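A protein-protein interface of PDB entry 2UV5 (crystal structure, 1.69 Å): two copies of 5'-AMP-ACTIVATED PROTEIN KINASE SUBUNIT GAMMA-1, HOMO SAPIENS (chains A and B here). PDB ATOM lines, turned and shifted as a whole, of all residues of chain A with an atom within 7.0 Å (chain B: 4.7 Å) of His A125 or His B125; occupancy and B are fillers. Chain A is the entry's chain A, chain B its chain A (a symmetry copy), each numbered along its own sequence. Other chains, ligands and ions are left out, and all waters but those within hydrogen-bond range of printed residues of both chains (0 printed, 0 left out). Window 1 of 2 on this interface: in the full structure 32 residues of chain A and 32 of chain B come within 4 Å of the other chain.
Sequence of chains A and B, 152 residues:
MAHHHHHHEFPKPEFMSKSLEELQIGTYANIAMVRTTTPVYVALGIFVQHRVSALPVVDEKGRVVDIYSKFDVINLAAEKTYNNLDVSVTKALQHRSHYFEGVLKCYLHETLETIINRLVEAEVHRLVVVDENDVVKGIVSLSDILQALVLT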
ATOM      1  N   SER A  69       9.729   9.455  -3.361  1.00  0.00           N
ATOM      2  CA  SER A  69      10.646  10.389  -2.728  1.00  0.00           C
ATOM      3  C   SER A  69      11.976  10.501  -3.456  1.00  0.00           C
ATOM      4  O   SER A  69      12.327   9.700  -4.350  1.00  0.00           O
ATOM      5  CB  SER A  69      10.933   9.940  -1.303  1.00  0.00           C
ATOM      6  OG  SER A  69      11.791   8.807  -1.272  1.00  0.00           O
ATOM      7  N   LYS A  70      12.747  11.481  -3.022  1.00  0.00           N
ATOM      8  CA  LYS A  70      14.109  11.657  -3.551  1.00  0.00           C
ATOM      9  C   LYS A  70      14.952  10.376  -3.350  1.00  0.00           C
ATOM     10  O   LYS A  70      15.748   9.984  -4.226  1.00  0.00           O
ATOM     11  CB  LYS A  70      14.752  12.882  -2.920  1.00  0.00           C
ATOM     12  CG  LYS A  70      14.145  14.198  -3.370  1.00  0.00           C
ATOM     13  CD  LYS A  70      14.841  15.415  -2.713  1.00  0.00           C
ATOM     14  CE  LYS A  70      14.472  16.738  -3.357  1.00  0.00           C
ATOM     15  NZ  LYS A  70      14.799  17.853  -2.421  1.00  0.00           N
ATOM     16  N   PHE A  71      14.789   9.710  -2.209  1.00  0.00           N
ATOM     17  CA  PHE A  71      15.541   8.495  -1.956  1.00  0.00           C
ATOM     18  C   PHE A  71      15.170   7.417  -2.971  1.00  0.00           C
ATOM     19  O   PHE A  71      16.037   6.703  -3.448  1.00  0.00           O
ATOM     20  CB  PHE A  71      15.376   7.962  -0.530  1.00  0.00           C
ATOM     21  CG  PHE A  71      16.186   6.719  -0.294  1.00  0.00           C
ATOM     22  CD1 PHE A  71      17.557   6.811  -0.077  1.00  0.00           C
ATOM     23  CD2 PHE A  71      15.597   5.465  -0.387  1.00  0.00           C
ATOM     24  CE1 PHE A  71      18.343   5.667   0.079  1.00  0.00           C
ATOM     25  CE2 PHE A  71      16.360   4.318  -0.221  1.00  0.00           C
ATOM     26  CZ  PHE A  71      17.749   4.422   0.005  1.00  0.00           C
ATOM     27  N   LEU A 119       5.267   6.642  11.926  1.00  0.00           N
ATOM     28  CA  LEU A 119       6.515   7.118  11.314  1.00  0.00           C
ATOM     29  C   LEU A 119       7.707   6.295  11.761  1.00  0.00           C
ATOM     30  O   LEU A 119       8.529   5.862  10.941  1.00  0.00           O
ATOM     31  CB  LEU A 119       6.741   8.614  11.636  1.00  0.00           C
ATOM     32  CG  LEU A 119       5.759   9.623  11.042  1.00  0.00           C
ATOM     33  CD1 LEU A 119       5.938  11.004  11.718  1.00  0.00           C
ATOM     34  CD2 LEU A 119       5.967   9.730   9.538  1.00  0.00           C
ATOM     35  N   ALA A 122       8.306   2.281  10.528  1.00  0.00           N
ATOM     36  CA  ALA A 122       8.951   1.972   9.241  1.00  0.00           C
ATOM     37  C   ALA A 122      10.086   2.928   8.891  1.00  0.00           C
ATOM     38  O   ALA A 122      10.604   2.885   7.788  1.00  0.00           O
ATOM     39  CB  ALA A 122       7.910   1.976   8.128  1.00  0.00           C
ATOM     40  N   GLU A 123      10.464   3.810   9.814  1.00  0.00           N
ATOM     41  CA  GLU A 123      11.437   4.829   9.512  1.00  0.00           C
ATOM     42  C   GLU A 123      11.057   5.548   8.203  1.00  0.00           C
ATOM     43  O   GLU A 123      11.830   5.584   7.247  1.00  0.00           O
ATOM     44  CB  GLU A 123      12.862   4.233   9.457  1.00  0.00           C
ATOM     45  CG  GLU A 123      13.874   5.129  10.170  1.00  0.00           C
ATOM     46  CD  GLU A 123      15.331   4.725   9.989  1.00  0.00           C
ATOM     47  OE1 GLU A 123      16.180   5.645   9.863  1.00  0.00           O
ATOM     48  OE2 GLU A 123      15.611   3.498   9.984  1.00  0.00           O
ATOM     49  N   VAL A 124       9.837   6.085   8.175  1.00  0.00           N
ATOM     50  CA  VAL A 124       9.380   6.954   7.089  1.00  0.00           C
ATOM     51  C   VAL A 124       9.275   8.393   7.590  1.00  0.00           C
ATOM     52  O   VAL A 124       9.121   8.638   8.783  1.00  0.00           O
ATOM     53  CB  VAL A 124       8.036   6.471   6.456  1.00  0.00           C
ATOM     54  CG1 VAL A 124       8.228   5.105   5.837  1.00  0.00           C
ATOM     55  CG2 VAL A 124       6.917   6.448   7.470  1.00  0.00           C
ATOM     56  N   HIS A 125       9.391   9.346   6.673  1.00  0.00           N
ATOM     57  CA  HIS A 125       9.558  10.750   7.049  1.00  0.00           C
ATOM     58  C   HIS A 125       8.316  11.610   6.800  1.00  0.00           C
ATOM     59  O   HIS A 125       8.329  12.817   7.041  1.00  0.00           O
ATOM     60  CB  HIS A 125      10.740  11.323   6.265  1.00  0.00           C
ATOM     61  CG  HIS A 125      12.059  10.749   6.680  1.00  0.00           C
ATOM     62  ND1 HIS A 125      13.259  11.241   6.217  1.00  0.00           N
ATOM     63  CD2 HIS A 125      12.368   9.737   7.529  1.00  0.00           C
ATOM     64  CE1 HIS A 125      14.250  10.542   6.750  1.00  0.00           C
ATOM     65  NE2 HIS A 125      13.736   9.624   7.548  1.00  0.00           N
ATOM     66  N   ARG A 126       7.266  10.984   6.274  1.00  0.00           N
ATOM     67  CA  ARG A 126       5.989  11.660   6.085  1.00  0.00           C
ATOM     68  C   ARG A 126       4.849  10.681   5.841  1.00  0.00           C
ATOM     69  O   ARG A 126       5.059   9.514   5.477  1.00  0.00           O
ATOM     70  CB  ARG A 126       6.028  12.655   4.914  1.00  0.00           C
ATOM     71  CG  ARG A 126       5.993  12.034   3.527  1.00  0.00           C
ATOM     72  CD  ARG A 126       7.299  11.411   3.088  1.00  0.00           C
ATOM     73  NE  ARG A 126       8.403  12.358   3.052  1.00  0.00           N
ATOM     74  CZ  ARG A 126       9.648  12.050   2.695  1.00  0.00           C
ATOM     75  NH1 ARG A 126       9.953  10.816   2.311  1.00  0.00           N
ATOM     76  NH2 ARG A 126      10.581  12.990   2.715  1.00  0.00           N
ATOM     77  N   LEU A 127       3.640  11.185   6.052  1.00  0.00           N
ATOM     78  CA  LEU A 127       2.413  10.461   5.735  1.00  0.00           C
ATOM     79  C   LEU A 127       1.443  11.349   4.955  1.00  0.00           C
ATOM     80  O   LEU A 127       1.410  12.563   5.129  1.00  0.00           O
ATOM     81  CB  LEU A 127       1.728   9.977   7.017  1.00  0.00           C
ATOM     82  CG  LEU A 127       2.529   8.957   7.874  1.00  0.00           C
ATOM     83  CD1 LEU A 127       1.974   8.963   9.319  1.00  0.00           C
ATOM     84  CD2 LEU A 127       2.503   7.548   7.309  1.00  0.00           C
ATOM     85  N   ILE A 139      -0.419  16.592   3.664  1.00  0.00           N
ATOM     86  CA  ILE A 139       0.791  15.903   4.036  1.00  0.00           C
ATOM     87  C   ILE A 139       1.235  16.329   5.426  1.00  0.00           C
ATOM     88  O   ILE A 139       1.200  17.535   5.781  1.00  0.00           O
ATOM     89  CB  ILE A 139       1.978  16.227   3.087  1.00  0.00           C
ATOM     90  CG1 ILE A 139       1.657  15.894   1.635  1.00  0.00           C
ATOM     91  CG2 ILE A 139       3.214  15.435   3.510  1.00  0.00           C
ATOM     92  CD1 ILE A 139       1.898  14.446   1.251  1.00  0.00           C
ATOM     93  N   VAL A 140       1.728  15.342   6.177  1.00  0.00           N
ATOM     94  CA  VAL A 140       2.395  15.593   7.468  1.00  0.00           C
ATOM     95  C   VAL A 140       3.789  14.986   7.425  1.00  0.00           C
ATOM     96  O   VAL A 140       3.938  13.770   7.245  1.00  0.00           O
ATOM     97  CB  VAL A 140       1.649  14.948   8.641  1.00  0.00           C
ATOM     98  CG1 VAL A 140       2.454  15.156   9.968  1.00  0.00           C
ATOM     99  CG2 VAL A 140       0.220  15.501   8.769  1.00  0.00           C
ATOM    100  N   SER A 141       4.800  15.826   7.553  1.00  0.00           N
ATOM    101  CA  SER A 141       6.186  15.376   7.536  1.00  0.00           C
ATOM    102  C   SER A 141       6.832  15.622   8.899  1.00  0.00           C
ATOM    103  O   SER A 141       6.240  16.251   9.810  1.00  0.00           O
ATOM    104  CB  SER A 141       6.970  16.140   6.464  1.00  0.00           C
ATOM    105  OG  SER A 141       7.057  17.485   6.860  1.00  0.00           O
ATOM    106  N   LEU A 142       8.071  15.172   9.039  1.00  0.00           N
ATOM    107  CA  LEU A 142       8.771  15.350  10.314  1.00  0.00           C
ATOM    108  C   LEU A 142       8.805  16.837  10.681  1.00  0.00           C
ATOM    109  O   LEU A 142       8.592  17.221  11.849  1.00  0.00           O
ATOM    110  CB  LEU A 142      10.202  14.811  10.222  1.00  0.00           C
ATOM    111  CG  LEU A 142      10.425  13.356   9.758  1.00  0.00           C
ATOM    112  CD1 LEU A 142      11.930  12.980   9.780  1.00  0.00           C
ATOM    113  CD2 LEU A 142       9.603  12.389  10.602  1.00  0.00           C
ATOM    114  N   SER A 143       9.058  17.691   9.684  1.00  0.00           N
ATOM    115  CA  SER A 143       9.120  19.136   9.933  1.00  0.00           C
ATOM    116  C   SER A 143       7.860  19.681  10.629  1.00  0.00           C
ATOM    117  O   SER A 143       7.934  20.461  11.594  1.00  0.00           O
ATOM    118  CB  SER A 143       9.402  19.865   8.633  1.00  0.00           C
ATOM    119  OG  SER A 143      10.662  19.430   8.141  1.00  0.00           O
ATOM    120  N   ILE A 145       5.703  17.987  12.440  1.00  0.00           N
ATOM    121  CA  ILE A 145       5.582  17.461  13.815  1.00  0.00           C
ATOM    122  C   ILE A 145       6.523  18.221  14.751  1.00  0.00           C
ATOM    123  O   ILE A 145       6.132  18.618  15.842  1.00  0.00           O
ATOM    124  CB  ILE A 145       5.838  15.962  13.851  1.00  0.00           C
ATOM    125  CG1 ILE A 145       4.688  15.240  13.128  1.00  0.00           C
ATOM    126  CG2 ILE A 145       5.999  15.444  15.315  1.00  0.00           C
ATOM    127  CD1 ILE A 145       5.109  13.954  12.527  1.00  0.00           C
ATOM    128  N   PHE B  71      14.500  12.966  12.120  1.00  0.00           N
ATOM    129  CA  PHE B  71      13.974  11.654  12.446  1.00  0.00           C
ATOM    130  C   PHE B  71      14.483  11.200  13.813  1.00  0.00           C
ATOM    131  O   PHE B  71      13.731  10.627  14.584  1.00  0.00           O
ATOM    132  CB  PHE B  71      14.282  10.593  11.386  1.00  0.00           C
ATOM    133  CG  PHE B  71      13.704   9.253  11.741  1.00  0.00           C
ATOM    134  CD1 PHE B  71      12.346   9.010  11.559  1.00  0.00           C
ATOM    135  CD2 PHE B  71      14.491   8.283  12.344  1.00  0.00           C
ATOM    136  CE1 PHE B  71      11.771   7.797  11.943  1.00  0.00           C
ATOM    137  CE2 PHE B  71      13.940   7.066  12.719  1.00  0.00           C
ATOM    138  CZ  PHE B  71      12.564   6.826  12.525  1.00  0.00           C
ATOM    139  N   LEU B 119      24.944   5.749   0.342  1.00  0.00           N
ATOM    140  CA  LEU B 119      23.610   6.225   0.736  1.00  0.00           C
ATOM    141  C   LEU B 119      22.592   5.101   0.735  1.00  0.00           C
ATOM    142  O   LEU B 119      21.824   4.933   1.692  1.00  0.00           O
ATOM    143  CB  LEU B 119      23.147   7.372  -0.192  1.00  0.00           C
ATOM    144  CG  LEU B 119      23.921   8.689  -0.131  1.00  0.00           C
ATOM    145  CD1 LEU B 119      23.538   9.590  -1.330  1.00  0.00           C
ATOM    146  CD2 LEU B 119      23.640   9.398   1.186  1.00  0.00           C
ATOM    147  N   GLU B 123      20.221   3.275   3.669  1.00  0.00           N
ATOM    148  CA  GLU B 123      19.079   4.144   3.539  1.00  0.00           C
ATOM    149  C   GLU B 123      19.282   5.411   4.392  1.00  0.00           C
ATOM    150  O   GLU B 123      18.477   5.725   5.268  1.00  0.00           O
ATOM    151  CB  GLU B 123      17.774   3.400   3.901  1.00  0.00           C
ATOM    152  CG  GLU B 123      16.653   3.715   2.910  1.00  0.00           C
ATOM    153  CD  GLU B 123      15.280   3.189   3.304  1.00  0.00           C
ATOM    154  OE1 GLU B 123      14.283   3.916   3.053  1.00  0.00           O
ATOM    155  OE2 GLU B 123      15.211   2.057   3.850  1.00  0.00           O
ATOM    156  N   VAL B 124      20.391   6.105   4.139  1.00  0.00           N
ATOM    157  CA  VAL B 124      20.652   7.421   4.724  1.00  0.00           C
ATOM    158  C   VAL B 124      20.533   8.497   3.647  1.00  0.00           C
ATOM    159  O   VAL B 124      20.689   8.225   2.460  1.00  0.00           O
ATOM    160  CB  VAL B 124      22.033   7.493   5.452  1.00  0.00           C
ATOM    161  CG1 VAL B 124      22.050   6.518   6.606  1.00  0.00           C
ATOM    162  CG2 VAL B 124      23.179   7.224   4.504  1.00  0.00           C
ATOM    163  N   HIS B 125      20.222   9.718   4.066  1.00  0.00           N
ATOM    164  CA  HIS B 125      19.835  10.771   3.127  1.00  0.00           C
ATOM    165  C   HIS B 125      20.903  11.851   2.932  1.00  0.00           C
ATOM    166  O   HIS B 125      20.697  12.813   2.194  1.00  0.00           O
ATOM    167  CB  HIS B 125      18.544  11.418   3.631  1.00  0.00           C
ATOM    168  CG  HIS B 125      17.358  10.508   3.557  1.00  0.00           C
ATOM    169  ND1 HIS B 125      16.075  10.942   3.808  1.00  0.00           N
ATOM    170  CD2 HIS B 125      17.257   9.193   3.240  1.00  0.00           C
ATOM    171  CE1 HIS B 125      15.237   9.924   3.668  1.00  0.00           C
ATOM    172  NE2 HIS B 125      15.929   8.853   3.325  1.00  0.00           N
ATOM    173  N   ARG B 126      22.023  11.700   3.636  1.00  0.00           N
ATOM    174  CA  ARG B 126      23.159  12.597   3.465  1.00  0.00           C
ATOM    175  C   ARG B 126      24.438  12.027   4.063  1.00  0.00           C
ATOM    176  O   ARG B 126      24.414  11.115   4.903  1.00  0.00           O
ATOM    177  CB  ARG B 126      22.908  13.977   4.091  1.00  0.00           C
ATOM    178  CG  ARG B 126      22.993  14.032   5.608  1.00  0.00           C
ATOM    179  CD  ARG B 126      21.795  13.450   6.323  1.00  0.00           C
ATOM    180  NE  ARG B 126      20.547  14.117   5.989  1.00  0.00           N
ATOM    181  CZ  ARG B 126      19.359  13.789   6.492  1.00  0.00           C
ATOM    182  NH1 ARG B 126      19.252  12.810   7.383  1.00  0.00           N
ATOM    183  NH2 ARG B 126      18.282  14.456   6.104  1.00  0.00           N
ATOM    184  N   VAL B 140      26.738  16.538   1.626  1.00  0.00           N
ATOM    185  CA  VAL B 140      26.089  16.089   0.381  1.00  0.00           C
ATOM    186  C   VAL B 140      24.817  15.335   0.736  1.00  0.00           C
ATOM    187  O   VAL B 140      24.868  14.311   1.428  1.00  0.00           O
ATOM    188  CB  VAL B 140      26.978  15.137  -0.427  1.00  0.00           C
ATOM    189  CG1 VAL B 140      26.201  14.613  -1.681  1.00  0.00           C
ATOM    190  CG2 VAL B 140      28.297  15.814  -0.836  1.00  0.00           C
ATOM    191  N   SER B 141      23.684  15.854   0.296  1.00  0.00           N
ATOM    192  CA  SER B 141      22.394  15.228   0.559  1.00  0.00           C
ATOM    193  C   SER B 141      21.769  14.749  -0.750  1.00  0.00           C
ATOM    194  O   SER B 141      22.281  15.012  -1.865  1.00  0.00           O
ATOM    195  CB  SER B 141      21.452  16.235   1.225  1.00  0.00           C
ATOM    196  OG  SER B 141      21.154  17.242   0.291  1.00  0.00           O
ATOM    197  N   LEU B 142      20.630  14.080  -0.634  1.00  0.00           N
ATOM    198  CA  LEU B 142      19.960  13.568  -1.833  1.00  0.00           C
ATOM    199  C   LEU B 142      19.690  14.722  -2.805  1.00  0.00           C
ATOM    200  O   LEU B 142      19.880  14.593  -4.031  1.00  0.00           O
ATOM    201  CB  LEU B 142      18.638  12.889  -1.462  1.00  0.00           C
ATOM    202  CG  LEU B 142      18.646  11.763  -0.406  1.00  0.00           C
ATOM    203  CD1 LEU B 142      17.228  11.167  -0.205  1.00  0.00           C
ATOM    204  CD2 LEU B 142      19.652  10.681  -0.781  1.00  0.00           C
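Phe A71 touches Glu B123, and with the chains exchanged Glu A123 touches Phe B71.
Phe A71 touches His B125, and with the chains exchanged His A125 touches Phe B71.
Phe A71 touches Leu B142, and with the chains exchanged Leu A142 touches Phe B71.
His B125 touches its own counterpart, His A125.
9 positions are printed for both chains.
Of the 10 pairs that touch across the chains among the printed residues, 9 have their exchanged pair printed and touching as well.
OG of Ser A69 lies close to N of Phe A71, at 3.3 Å.
The backbone NH of Val A124 sits at hydrogen-bond distance from the backbone carbonyl oxygen of Leu A119, at 3.1 Å.
O of His A125 sits at hydrogen-bond distance from N of Leu A142 (3.1 Å).
The backbone carbonyl oxygen (O) of Leu B119 lies within hydrogen-bond range of the backbone NH (N) of Val B124 (3.1 Å).
O of His B125 lies within hydrogen-bond range of N of Leu B142 (3.1 Å).
Hydrophobic or aromatic side chains of chain A within 4 Å of the printed part of chain B: Phe A71, His A125 and Leu A142.
Among the printed residues, no Asp or Glu carboxylate lies within 4 Å of a Lys or Arg side-chain nitrogen of the other chain.
Lys A70 touches Leu B142.
O of Leu B119 touches CE1 of Phe A71, 3.9 Å away.
Phe A71 touches Glu B123.
Phe A71 touches His B125.
Phe A71 touches Leu B142.
Leu A119 touches Phe B71.
CG of Glu A123 touches CZ of Phe B71, at 3.2 Å.
His A125 touches Phe B71.
His A125 touches His B125.
CD1 of Leu A142 touches N of Phe B71 (3.5 Å).
Ser A69 touches none of the printed residues of chain B.
Printed residues of chain B within 4 Å of Leu A119: Phe B71.
Of the printed residues of chain B, His A125 touches Phe B71 (3.996 Å) and His B125 (3.3 Å).
Of the printed residues of chain A, His B125 touches Phe A71 (3.995 Å) and His A125 (3.3 Å).
Ser B141 touches none of the printed residues of chain A.
Of the printed residues of chain A, Leu B142 touches Lys A70 and Phe A71.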
